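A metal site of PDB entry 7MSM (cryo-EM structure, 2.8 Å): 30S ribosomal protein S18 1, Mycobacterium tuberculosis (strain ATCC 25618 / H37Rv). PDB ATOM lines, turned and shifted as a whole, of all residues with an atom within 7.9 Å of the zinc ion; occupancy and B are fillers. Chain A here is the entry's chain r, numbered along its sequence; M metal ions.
N of Gln 59 lies close to SG of Cys 57 (3.7 Å).
The zinc ion is bound by ND1 of His 60 (2.2 Å), SG of Cys 23 (2.4 Å), SG of Cys 57 (2.4 Å) and SG of Cys 20 (2.5 Å). The zinc ion has four donor atoms within binding distance.
The nearest printed residue that does not touch the zinc ion is Phe 22 (4.2 Å).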
ATOM      1  N   LYS A  19      19.892   6.847   7.627  1.00  0.00           N
ATOM      2  CA  LYS A  19      18.941   5.842   8.066  1.00  0.00           C
ATOM      3  C   LYS A  19      19.678   4.516   8.097  1.00  0.00           C
ATOM      4  O   LYS A  19      19.323   3.604   8.838  1.00  0.00           O
ATOM      5  CB  LYS A  19      17.736   5.803   7.120  1.00  0.00           C
ATOM      6  CG  LYS A  19      16.493   5.125   7.684  1.00  0.00           C
ATOM      7  CD  LYS A  19      16.366   3.665   7.265  1.00  0.00           C
ATOM      8  CE  LYS A  19      15.029   3.090   7.715  1.00  0.00           C
ATOM      9  NZ  LYS A  19      14.944   3.036   9.187  1.00  0.00           N
ATOM     10  N   CYS A  20      20.730   4.432   7.283  1.00  0.00           N
ATOM     11  CA  CYS A  20      21.662   3.312   7.322  1.00  0.00           C
ATOM     12  C   CYS A  20      22.795   3.632   8.285  1.00  0.00           C
ATOM     13  O   CYS A  20      23.426   4.687   8.163  1.00  0.00           O
ATOM     14  CB  CYS A  20      22.222   3.034   5.925  1.00  0.00           C
ATOM     15  SG  CYS A  20      23.369   1.666   5.839  1.00  0.00           S
ATOM     16  N   VAL A  21      23.046   2.735   9.233  1.00  0.00           N
ATOM     17  CA  VAL A  21      24.021   3.011  10.272  1.00  0.00           C
ATOM     18  C   VAL A  21      25.434   2.961   9.718  1.00  0.00           C
ATOM     19  O   VAL A  21      26.286   3.787  10.051  1.00  0.00           O
ATOM     20  CB  VAL A  21      23.837   2.035  11.445  1.00  0.00           C
ATOM     21  CG1 VAL A  21      24.837   2.315  12.550  1.00  0.00           C
ATOM     22  CG2 VAL A  21      22.429   2.103  11.978  1.00  0.00           C
ATOM     23  N   PHE A  22      25.699   2.017   8.824  1.00  0.00           N
ATOM     24  CA  PHE A  22      27.049   1.823   8.320  1.00  0.00           C
ATOM     25  C   PHE A  22      27.465   2.873   7.295  1.00  0.00           C
ATOM     26  O   PHE A  22      28.656   3.117   7.131  1.00  0.00           O
ATOM     27  CB  PHE A  22      27.194   0.436   7.726  1.00  0.00           C
ATOM     28  CG  PHE A  22      27.048  -0.650   8.729  1.00  0.00           C
ATOM     29  CD1 PHE A  22      28.085  -0.944   9.592  1.00  0.00           C
ATOM     30  CD2 PHE A  22      25.885  -1.393   8.809  1.00  0.00           C
ATOM     31  CE1 PHE A  22      27.955  -1.937  10.518  1.00  0.00           C
ATOM     32  CE2 PHE A  22      25.768  -2.396   9.729  1.00  0.00           C
ATOM     33  CZ  PHE A  22      26.803  -2.668  10.584  1.00  0.00           C
ATOM     34  N   CYS A  23      26.509   3.489   6.587  1.00  0.00           N
ATOM     35  CA  CYS A  23      26.867   4.626   5.747  1.00  0.00           C
ATOM     36  C   CYS A  23      27.019   5.902   6.546  1.00  0.00           C
ATOM     37  O   CYS A  23      27.831   6.758   6.191  1.00  0.00           O
ATOM     38  CB  CYS A  23      25.835   4.844   4.637  1.00  0.00           C
ATOM     39  SG  CYS A  23      25.820   3.621   3.319  1.00  0.00           S
ATOM     40  N   ALA A  24      26.253   6.046   7.633  1.00  0.00           N
ATOM     41  CA  ALA A  24      26.339   7.255   8.443  1.00  0.00           C
ATOM     42  C   ALA A  24      27.631   7.288   9.244  1.00  0.00           C
ATOM     43  O   ALA A  24      28.475   8.172   9.064  1.00  0.00           O
ATOM     44  CB  ALA A  24      25.131   7.353   9.373  1.00  0.00           C
ATOM     45  N   ILE A  30      32.532  -4.103   9.345  1.00  0.00           N
ATOM     46  CA  ILE A  30      31.769  -5.324   9.509  1.00  0.00           C
ATOM     47  C   ILE A  30      32.737  -6.501   9.469  1.00  0.00           C
ATOM     48  O   ILE A  30      33.408  -6.727   8.459  1.00  0.00           O
ATOM     49  CB  ILE A  30      30.715  -5.444   8.415  1.00  0.00           C
ATOM     50  CG1 ILE A  30      29.722  -4.295   8.520  1.00  0.00           C
ATOM     51  CG2 ILE A  30      30.001  -6.757   8.522  1.00  0.00           C
ATOM     52  CD1 ILE A  30      28.858  -4.135   7.325  1.00  0.00           C
ATOM     53  N   GLY A  55      17.193  -1.180   7.402  1.00  0.00           N
ATOM     54  CA  GLY A  55      17.587   0.117   6.890  1.00  0.00           C
ATOM     55  C   GLY A  55      18.934   0.165   6.224  1.00  0.00           C
ATOM     56  O   GLY A  55      19.405   1.264   5.901  1.00  0.00           O
ATOM     57  N   ASN A  56      19.565  -0.982   5.985  1.00  0.00           N
ATOM     58  CA  ASN A  56      20.853  -1.006   5.319  1.00  0.00           C
ATOM     59  C   ASN A  56      20.717  -0.666   3.840  1.00  0.00           C
ATOM     60  O   ASN A  56      19.644  -0.806   3.238  1.00  0.00           O
ATOM     61  CB  ASN A  56      21.501  -2.383   5.437  1.00  0.00           C
ATOM     62  CG  ASN A  56      21.959  -2.693   6.840  1.00  0.00           C
ATOM     63  OD1 ASN A  56      22.519  -1.847   7.518  1.00  0.00           O
ATOM     64  ND2 ASN A  56      21.723  -3.916   7.274  1.00  0.00           N
ATOM     65  N   CYS A  57      21.815  -0.235   3.245  1.00  0.00           N
ATOM     66  CA  CYS A  57      21.910  -0.127   1.803  1.00  0.00           C
ATOM     67  C   CYS A  57      22.188  -1.500   1.215  1.00  0.00           C
ATOM     68  O   CYS A  57      22.294  -2.496   1.938  1.00  0.00           O
ATOM     69  CB  CYS A  57      22.993   0.874   1.421  1.00  0.00           C
ATOM     70  SG  CYS A  57      24.653   0.409   1.928  1.00  0.00           S
ATOM     71  N   VAL A  58      22.278  -1.581  -0.107  1.00  0.00           N
ATOM     72  CA  VAL A  58      22.493  -2.865  -0.766  1.00  0.00           C
ATOM     73  C   VAL A  58      23.893  -3.385  -0.484  1.00  0.00           C
ATOM     74  O   VAL A  58      24.097  -4.580  -0.279  1.00  0.00           O
ATOM     75  CB  VAL A  58      22.256  -2.735  -2.280  1.00  0.00           C
ATOM     76  CG1 VAL A  58      22.388  -4.075  -2.969  1.00  0.00           C
ATOM     77  CG2 VAL A  58      20.911  -2.161  -2.559  1.00  0.00           C
ATOM     78  N   GLN A  59      24.873  -2.480  -0.441  1.00  0.00           N
ATOM     79  CA  GLN A  59      26.256  -2.883  -0.299  1.00  0.00           C
ATOM     80  C   GLN A  59      26.554  -3.366   1.114  1.00  0.00           C
ATOM     81  O   GLN A  59      27.335  -4.301   1.305  1.00  0.00           O
ATOM     82  CB  GLN A  59      27.175  -1.730  -0.656  1.00  0.00           C
ATOM     83  CG  GLN A  59      27.038  -1.276  -2.065  1.00  0.00           C
ATOM     84  CD  GLN A  59      27.957  -0.136  -2.347  1.00  0.00           C
ATOM     85  OE1 GLN A  59      28.682   0.317  -1.474  1.00  0.00           O
ATOM     86  NE2 GLN A  59      27.926   0.362  -3.568  1.00  0.00           N
ATOM     87  N   HIS A  60      25.956  -2.728   2.120  1.00  0.00           N
ATOM     88  CA  HIS A  60      26.211  -3.161   3.471  1.00  0.00           C
ATOM     89  C   HIS A  60      25.348  -4.337   3.887  1.00  0.00           C
ATOM     90  O   HIS A  60      25.714  -5.039   4.825  1.00  0.00           O
ATOM     91  CB  HIS A  60      26.040  -2.022   4.462  1.00  0.00           C
ATOM     92  CG  HIS A  60      27.077  -0.960   4.351  1.00  0.00           C
ATOM     93  ND1 HIS A  60      26.863   0.228   3.691  1.00  0.00           N
ATOM     94  CD2 HIS A  60      28.368  -0.941   4.749  1.00  0.00           C
ATOM     95  CE1 HIS A  60      27.958   0.962   3.737  1.00  0.00           C
ATOM     96  NE2 HIS A  60      28.888   0.275   4.378  1.00  0.00           N
ATOM     97  N   GLN A  61      24.223  -4.572   3.219  1.00  0.00           N
ATOM     98  CA  GLN A  61      23.495  -5.809   3.455  1.00  0.00           C
ATOM     99  C   GLN A  61      24.264  -7.008   2.919  1.00  0.00           C
ATOM    100  O   GLN A  61      24.163  -8.106   3.475  1.00  0.00           O
ATOM    101  CB  GLN A  61      22.109  -5.724   2.838  1.00  0.00           C
ATOM    102  CG  GLN A  61      21.205  -6.896   3.124  1.00  0.00           C
ATOM    103  CD  GLN A  61      20.849  -7.003   4.580  1.00  0.00           C
ATOM    104  OE1 GLN A  61      20.623  -6.006   5.245  1.00  0.00           O
ATOM    105  NE2 GLN A  61      20.783  -8.226   5.075  1.00  0.00           N
HETATM  106 ZN    ZN M   1      25.104   1.436   4.106  1.00  0.00          ZN
